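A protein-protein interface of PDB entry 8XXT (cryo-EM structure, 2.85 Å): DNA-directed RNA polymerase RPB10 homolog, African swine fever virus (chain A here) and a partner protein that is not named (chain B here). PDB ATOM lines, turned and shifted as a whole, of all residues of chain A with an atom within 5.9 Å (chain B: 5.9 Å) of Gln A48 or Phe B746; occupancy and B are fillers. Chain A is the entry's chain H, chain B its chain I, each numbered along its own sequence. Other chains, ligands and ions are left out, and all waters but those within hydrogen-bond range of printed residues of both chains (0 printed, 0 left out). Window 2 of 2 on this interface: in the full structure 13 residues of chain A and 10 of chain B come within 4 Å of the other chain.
The backbone NH (N) of Gln B740 sits at hydrogen-bond distance from the backbone carbonyl oxygen (O) of Ser A46 (2.7 Å). O of Ser A46 is in hydrogen-bond range of N of Gly B741, at 3.0 Å. The backbone carbonyl oxygen of Phe B742 lies within hydrogen-bond range of the backbone NH of Ser A46 (3.2 Å). The backbone NH (N) of Leu A47 sits at hydrogen-bond distance from the backbone carbonyl oxygen (O) of Phe B742 (3.3 Å). The backbone carbonyl oxygen (O) of Gln B740 is in hydrogen-bond range of the backbone NH (N) of Gln A48, 3.1 Å away. The backbone NH (N) of Tyr B743 lies close to the side-chain amide nitrogen (NE2) of Gln A48 (3.0 Å). The backbone NH (N) of Phe B742 lies close to the backbone NH (N) of Gln A48.
Of the 15 printed residues of chain B, 6 touch a printed residue of chain A. Hydrophobic or aromatic side chains of chain B within 4 Å of the printed part of chain A: Phe B742, Tyr B743 and Phe B746. Along chain B the printed residues that touch a printed residue of chain A span positions 740 to 746. Among the printed residues, 15 pairs touch across the chains. Among the printed residues, no Asp or Glu carboxylate lies within 4 Å of a Lys or Arg side-chain nitrogen of the other chain.
Leu A47 touches Gln B740. N of Leu A47 touches C of Gly B741, at 3.6 Å. Leu A47 touches Tyr B743 (O to CD2, 3.0 Å). CA of Gly B741 touches N of Gln A48, at 3.1 Å. OE1 of Gln A48 touches N of Asn B744 (3.9 Å). CZ of Phe B746 touches OE1 of Gln A48, at 3.8 Å. CG1 of Ile A49 touches O of Gln B740, 3.4 Å away. Ile A49 touches Tyr B743 (O to CD2, 3.8 Å).
Printed residues of chain B within 4 Å of Ser A46: Gln B740, Gly B741 and Phe B742. Of chain B, only Gln B740 (3.1 Å), Gly B741 (3.1 Å), Phe B742 (3.0 Å), Tyr B743 (3.0 Å), Asn B744 (3.9 Å) and Phe B746 (3.8 Å) come within 4 Å of Gln A48. Printed residues of chain A within 4 Å of Gly B741: Ser A46 (3.0 Å), Leu A47 (3.6 Å) and Gln A48 (3.1 Å). Of the printed residues of chain A, Phe B742 touches Ser A46, Leu A47 and Gln A48. Printed residues of chain A within 4 Å of Asn B744: Gln A48. Printed residues of chain A within 4 Å of Phe B746: Gln A48 (3.8 Å). Asp B747 touches none of the printed residues of chain A. Thr B750 touches none of the printed residues of chain A. The nearest printed residue of chain A that does not touch Phe B746 is Glu A50 (6.5 Å). The nearest printed residue of chain A that does not touch Asn B744 is Leu A47 (5.9 Å).
N of Asp B754 lies within hydrogen-bond range of OD1 of Asn B744, 3.3 Å away.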
ATOM      1  N   LYS A  32       3.713   7.830  -2.256  1.00  0.00           N
ATOM      2  CA  LYS A  32       3.841   8.666  -1.067  1.00  0.00           C
ATOM      3  C   LYS A  32       2.989   9.924  -1.178  1.00  0.00           C
ATOM      4  O   LYS A  32       2.533  10.460  -0.162  1.00  0.00           O
ATOM      5  CB  LYS A  32       5.311   9.024  -0.826  1.00  0.00           C
ATOM      6  CG  LYS A  32       5.557   9.929   0.374  1.00  0.00           C
ATOM      7  CD  LYS A  32       4.925   9.372   1.642  1.00  0.00           C
ATOM      8  CE  LYS A  32       5.793   9.624   2.864  1.00  0.00           C
ATOM      9  NZ  LYS A  32       6.739   8.505   3.126  1.00  0.00           N
ATOM     10  N   SER A  46       6.645  19.944  -2.156  1.00  0.00           N
ATOM     11  CA  SER A  46       7.952  19.685  -2.774  1.00  0.00           C
ATOM     12  C   SER A  46       8.421  18.229  -2.748  1.00  0.00           C
ATOM     13  O   SER A  46       8.498  17.586  -3.799  1.00  0.00           O
ATOM     14  CB  SER A  46       8.996  20.597  -2.129  1.00  0.00           C
ATOM     15  OG  SER A  46       8.670  21.958  -2.349  1.00  0.00           O
ATOM     16  N   LEU A  47       8.778  17.707  -1.573  1.00  0.00           N
ATOM     17  CA  LEU A  47       9.650  16.530  -1.559  1.00  0.00           C
ATOM     18  C   LEU A  47       9.336  15.626  -0.355  1.00  0.00           C
ATOM     19  O   LEU A  47      10.183  15.382   0.501  1.00  0.00           O
ATOM     20  CB  LEU A  47      11.113  16.978  -1.618  1.00  0.00           C
ATOM     21  CG  LEU A  47      12.414  16.140  -1.650  1.00  0.00           C
ATOM     22  CD1 LEU A  47      12.789  15.274  -0.466  1.00  0.00           C
ATOM     23  CD2 LEU A  47      12.506  15.355  -2.959  1.00  0.00           C
ATOM     24  N   GLN A  48       8.087  15.169  -0.211  1.00  0.00           N
ATOM     25  CA  GLN A  48       7.702  14.414   0.991  1.00  0.00           C
ATOM     26  C   GLN A  48       8.525  13.142   1.211  1.00  0.00           C
ATOM     27  O   GLN A  48       8.303  12.442   2.205  1.00  0.00           O
ATOM     28  CB  GLN A  48       6.210  14.045   0.931  1.00  0.00           C
ATOM     29  CG  GLN A  48       5.549  13.645   2.257  1.00  0.00           C
ATOM     30  CD  GLN A  48       5.697  14.690   3.342  1.00  0.00           C
ATOM     31  OE1 GLN A  48       6.643  14.652   4.126  1.00  0.00           O
ATOM     32  NE2 GLN A  48       4.753  15.617   3.407  1.00  0.00           N
ATOM     33  N   ILE A  49       9.484  12.847   0.348  1.00  0.00           N
ATOM     34  CA  ILE A  49      10.128  11.552   0.318  1.00  0.00           C
ATOM     35  C   ILE A  49      11.412  11.613   1.133  1.00  0.00           C
ATOM     36  O   ILE A  49      11.874  12.680   1.545  1.00  0.00           O
ATOM     37  CB  ILE A  49      10.453  11.142  -1.123  1.00  0.00           C
ATOM     38  CG1 ILE A  49      10.920  12.369  -1.884  1.00  0.00           C
ATOM     39  CG2 ILE A  49       9.189  10.711  -1.819  1.00  0.00           C
ATOM     40  CD1 ILE A  49      11.233  12.106  -3.310  1.00  0.00           C
ATOM     41  N   GLU A  50      11.991  10.441   1.380  1.00  0.00           N
ATOM     42  CA  GLU A  50      13.410  10.293   1.674  1.00  0.00           C
ATOM     43  C   GLU A  50      13.972   9.269   0.699  1.00  0.00           C
ATOM     44  O   GLU A  50      13.479   8.140   0.634  1.00  0.00           O
ATOM     45  CB  GLU A  50      13.663   9.848   3.115  1.00  0.00           C
ATOM     46  CG  GLU A  50      12.878  10.613   4.159  1.00  0.00           C
ATOM     47  CD  GLU A  50      12.230   9.700   5.179  1.00  0.00           C
ATOM     48  OE1 GLU A  50      11.524   8.756   4.767  1.00  0.00           O
ATOM     49  OE2 GLU A  50      12.434   9.924   6.390  1.00  0.00           O
ATOM     50  N   GLN B 740       7.938  16.105  -6.044  1.00  0.00           N
ATOM     51  CA  GLN B 740       8.331  14.882  -5.352  1.00  0.00           C
ATOM     52  C   GLN B 740       7.715  14.753  -3.955  1.00  0.00           C
ATOM     53  O   GLN B 740       8.298  14.098  -3.082  1.00  0.00           O
ATOM     54  CB  GLN B 740       9.858  14.798  -5.256  1.00  0.00           C
ATOM     55  CG  GLN B 740      10.539  14.153  -6.459  1.00  0.00           C
ATOM     56  CD  GLN B 740      11.269  15.146  -7.342  1.00  0.00           C
ATOM     57  OE1 GLN B 740      12.208  15.809  -6.908  1.00  0.00           O
ATOM     58  NE2 GLN B 740      10.856  15.228  -8.600  1.00  0.00           N
ATOM     59  N   GLY B 741       6.542  15.339  -3.720  1.00  0.00           N
ATOM     60  CA  GLY B 741       5.871  15.167  -2.440  1.00  0.00           C
ATOM     61  C   GLY B 741       5.372  16.449  -1.803  1.00  0.00           C
ATOM     62  O   GLY B 741       4.784  17.269  -2.506  1.00  0.00           O
ATOM     63  N   PHE B 742       5.486  16.587  -0.475  1.00  0.00           N
ATOM     64  CA  PHE B 742       5.334  17.866   0.218  1.00  0.00           C
ATOM     65  C   PHE B 742       6.539  18.209   1.100  1.00  0.00           C
ATOM     66  O   PHE B 742       7.208  19.227   0.892  1.00  0.00           O
ATOM     67  CB  PHE B 742       4.055  17.837   1.065  1.00  0.00           C
ATOM     68  CG  PHE B 742       3.773  19.117   1.804  1.00  0.00           C
ATOM     69  CD1 PHE B 742       3.439  20.270   1.120  1.00  0.00           C
ATOM     70  CD2 PHE B 742       3.839  19.160   3.185  1.00  0.00           C
ATOM     71  CE1 PHE B 742       3.179  21.445   1.798  1.00  0.00           C
ATOM     72  CE2 PHE B 742       3.580  20.329   3.869  1.00  0.00           C
ATOM     73  CZ  PHE B 742       3.250  21.473   3.174  1.00  0.00           C
ATOM     74  N   TYR B 743       6.808  17.342   2.086  1.00  0.00           N
ATOM     75  CA  TYR B 743       7.921  17.388   3.041  1.00  0.00           C
ATOM     76  C   TYR B 743       7.793  18.446   4.135  1.00  0.00           C
ATOM     77  O   TYR B 743       7.336  19.567   3.889  1.00  0.00           O
ATOM     78  CB  TYR B 743       9.277  17.573   2.351  1.00  0.00           C
ATOM     79  CG  TYR B 743      10.415  17.186   3.272  1.00  0.00           C
ATOM     80  CD1 TYR B 743      11.003  18.117   4.109  1.00  0.00           C
ATOM     81  CD2 TYR B 743      10.856  15.875   3.349  1.00  0.00           C
ATOM     82  CE1 TYR B 743      12.013  17.764   4.974  1.00  0.00           C
ATOM     83  CE2 TYR B 743      11.871  15.511   4.209  1.00  0.00           C
ATOM     84  CZ  TYR B 743      12.445  16.461   5.020  1.00  0.00           C
ATOM     85  OH  TYR B 743      13.457  16.111   5.882  1.00  0.00           O
ATOM     86  N   ASN B 744       8.191  18.070   5.352  1.00  0.00           N
ATOM     87  CA  ASN B 744       8.672  19.004   6.362  1.00  0.00           C
ATOM     88  C   ASN B 744       9.397  18.186   7.423  1.00  0.00           C
ATOM     89  O   ASN B 744       9.200  16.974   7.530  1.00  0.00           O
ATOM     90  CB  ASN B 744       7.541  19.830   6.983  1.00  0.00           C
ATOM     91  CG  ASN B 744       8.055  20.874   7.953  1.00  0.00           C
ATOM     92  OD1 ASN B 744       8.020  20.686   9.164  1.00  0.00           O
ATOM     93  ND2 ASN B 744       8.529  21.994   7.418  1.00  0.00           N
ATOM     94  N   ILE B 745      10.250  18.856   8.202  1.00  0.00           N
ATOM     95  CA  ILE B 745      10.910  18.196   9.325  1.00  0.00           C
ATOM     96  C   ILE B 745       9.896  17.973  10.437  1.00  0.00           C
ATOM     97  O   ILE B 745       9.196  18.903  10.853  1.00  0.00           O
ATOM     98  CB  ILE B 745      12.107  19.023   9.819  1.00  0.00           C
ATOM     99  CG1 ILE B 745      13.300  18.872   8.876  1.00  0.00           C
ATOM    100  CG2 ILE B 745      12.500  18.614  11.228  1.00  0.00           C
ATOM    101  CD1 ILE B 745      14.450  19.796   9.205  1.00  0.00           C
ATOM    102  N   PHE B 746       9.817  16.741  10.930  1.00  0.00           N
ATOM    103  CA  PHE B 746       8.781  16.363  11.883  1.00  0.00           C
ATOM    104  C   PHE B 746       9.281  16.503  13.315  1.00  0.00           C
ATOM    105  O   PHE B 746      10.393  16.077  13.639  1.00  0.00           O
ATOM    106  CB  PHE B 746       8.313  14.931  11.628  1.00  0.00           C
ATOM    107  CG  PHE B 746       7.604  14.750  10.321  1.00  0.00           C
ATOM    108  CD1 PHE B 746       6.304  15.189  10.159  1.00  0.00           C
ATOM    109  CD2 PHE B 746       8.240  14.141   9.251  1.00  0.00           C
ATOM    110  CE1 PHE B 746       5.648  15.025   8.958  1.00  0.00           C
ATOM    111  CE2 PHE B 746       7.590  13.976   8.046  1.00  0.00           C
ATOM    112  CZ  PHE B 746       6.291  14.419   7.901  1.00  0.00           C
ATOM    113  N   ASP B 747       8.453  17.107  14.159  1.00  0.00           N
ATOM    114  CA  ASP B 747       8.726  17.199  15.587  1.00  0.00           C
ATOM    115  C   ASP B 747       8.365  15.878  16.257  1.00  0.00           C
ATOM    116  O   ASP B 747       7.237  15.403  16.091  1.00  0.00           O
ATOM    117  CB  ASP B 747       7.919  18.344  16.190  1.00  0.00           C
ATOM    118  CG  ASP B 747       8.199  18.561  17.661  1.00  0.00           C
ATOM    119  OD1 ASP B 747       9.152  17.964  18.195  1.00  0.00           O
ATOM    120  OD2 ASP B 747       7.459  19.344  18.289  1.00  0.00           O
ATOM    121  N   PRO B 748       9.285  15.235  16.979  1.00  0.00           N
ATOM    122  CA  PRO B 748       8.915  13.998  17.685  1.00  0.00           C
ATOM    123  C   PRO B 748       7.821  14.189  18.724  1.00  0.00           C
ATOM    124  O   PRO B 748       6.995  13.286  18.907  1.00  0.00           O
ATOM    125  CB  PRO B 748      10.236  13.552  18.326  1.00  0.00           C
ATOM    126  CG  PRO B 748      11.093  14.772  18.345  1.00  0.00           C
ATOM    127  CD  PRO B 748      10.718  15.538  17.121  1.00  0.00           C
ATOM    128  N   THR B 750       5.271  16.459  18.705  1.00  0.00           N
ATOM    129  CA  THR B 750       4.040  16.590  17.930  1.00  0.00           C
ATOM    130  C   THR B 750       4.359  16.194  16.496  1.00  0.00           C
ATOM    131  O   THR B 750       5.009  16.954  15.771  1.00  0.00           O
ATOM    132  CB  THR B 750       3.486  18.014  17.993  1.00  0.00           C
ATOM    133  OG1 THR B 750       4.451  18.929  17.460  1.00  0.00           O
ATOM    134  CG2 THR B 750       3.175  18.400  19.427  1.00  0.00           C
ATOM    135  N   GLY B 751       3.873  15.033  16.071  1.00  0.00           N
ATOM    136  CA  GLY B 751       4.346  14.422  14.845  1.00  0.00           C
ATOM    137  C   GLY B 751       3.959  15.133  13.564  1.00  0.00           C
ATOM    138  O   GLY B 751       4.001  14.540  12.483  1.00  0.00           O
ATOM    139  N   ARG B 752       3.570  16.397  13.676  1.00  0.00           N
ATOM    140  CA  ARG B 752       3.323  17.254  12.525  1.00  0.00           C
ATOM    141  C   ARG B 752       4.605  18.022  12.194  1.00  0.00           C
ATOM    142  O   ARG B 752       5.697  17.646  12.628  1.00  0.00           O
ATOM    143  CB  ARG B 752       2.134  18.176  12.801  1.00  0.00           C
ATOM    144  CG  ARG B 752       0.795  17.462  12.819  1.00  0.00           C
ATOM    145  CD  ARG B 752      -0.287  18.343  13.421  1.00  0.00           C
ATOM    146  NE  ARG B 752      -0.297  18.301  14.877  1.00  0.00           N
ATOM    147  CZ  ARG B 752       0.263  19.216  15.654  1.00  0.00           C
ATOM    148  NH1 ARG B 752       0.897  20.259  15.146  1.00  0.00           N
ATOM    149  NH2 ARG B 752       0.185  19.084  16.975  1.00  0.00           N
ATOM    150  N   ALA B 753       4.488  19.079  11.395  1.00  0.00           N
ATOM    151  CA  ALA B 753       5.629  19.929  11.081  1.00  0.00           C
ATOM    152  C   ALA B 753       6.263  20.489  12.351  1.00  0.00           C
ATOM    153  O   ALA B 753       5.568  20.907  13.281  1.00  0.00           O
ATOM    154  CB  ALA B 753       5.185  21.074  10.170  1.00  0.00           C
ATOM    155  N   ASP B 754       7.594  20.499  12.383  1.00  0.00           N
ATOM    156  CA  ASP B 754       8.322  20.971  13.556  1.00  0.00           C
ATOM    157  C   ASP B 754       8.227  22.486  13.651  1.00  0.00           C
ATOM    158  O   ASP B 754       8.587  23.200  12.711  1.00  0.00           O
ATOM    159  CB  ASP B 754       9.781  20.525  13.486  1.00  0.00           C
ATOM    160  CG  ASP B 754      10.506  20.668  14.814  1.00  0.00           C
ATOM    161  OD1 ASP B 754      10.028  21.419  15.689  1.00  0.00           O
ATOM    162  OD2 ASP B 754      11.557  20.015  14.985  1.00  0.00           O
ATOM    163  N   ARG B 756       9.349  24.111  16.680  1.00  0.00           N
ATOM    164  CA  ARG B 756      10.183  24.548  17.792  1.00  0.00           C
ATOM    165  C   ARG B 756      11.141  25.643  17.345  1.00  0.00           C
ATOM    166  O   ARG B 756      11.764  25.551  16.286  1.00  0.00           O
ATOM    167  CB  ARG B 756      10.967  23.370  18.367  1.00  0.00           C
ATOM    168  CG  ARG B 756      10.115  22.346  19.087  1.00  0.00           C
ATOM    169  CD  ARG B 756      10.916  21.094  19.385  1.00  0.00           C
ATOM    170  NE  ARG B 756      11.350  20.425  18.166  1.00  0.00           N
ATOM    171  CZ  ARG B 756      12.011  19.278  18.139  1.00  0.00           C
ATOM    172  NH1 ARG B 756      12.322  18.632  19.251  1.00  0.00           N
ATOM    173  NH2 ARG B 756      12.373  18.765  16.967  1.00  0.00           N
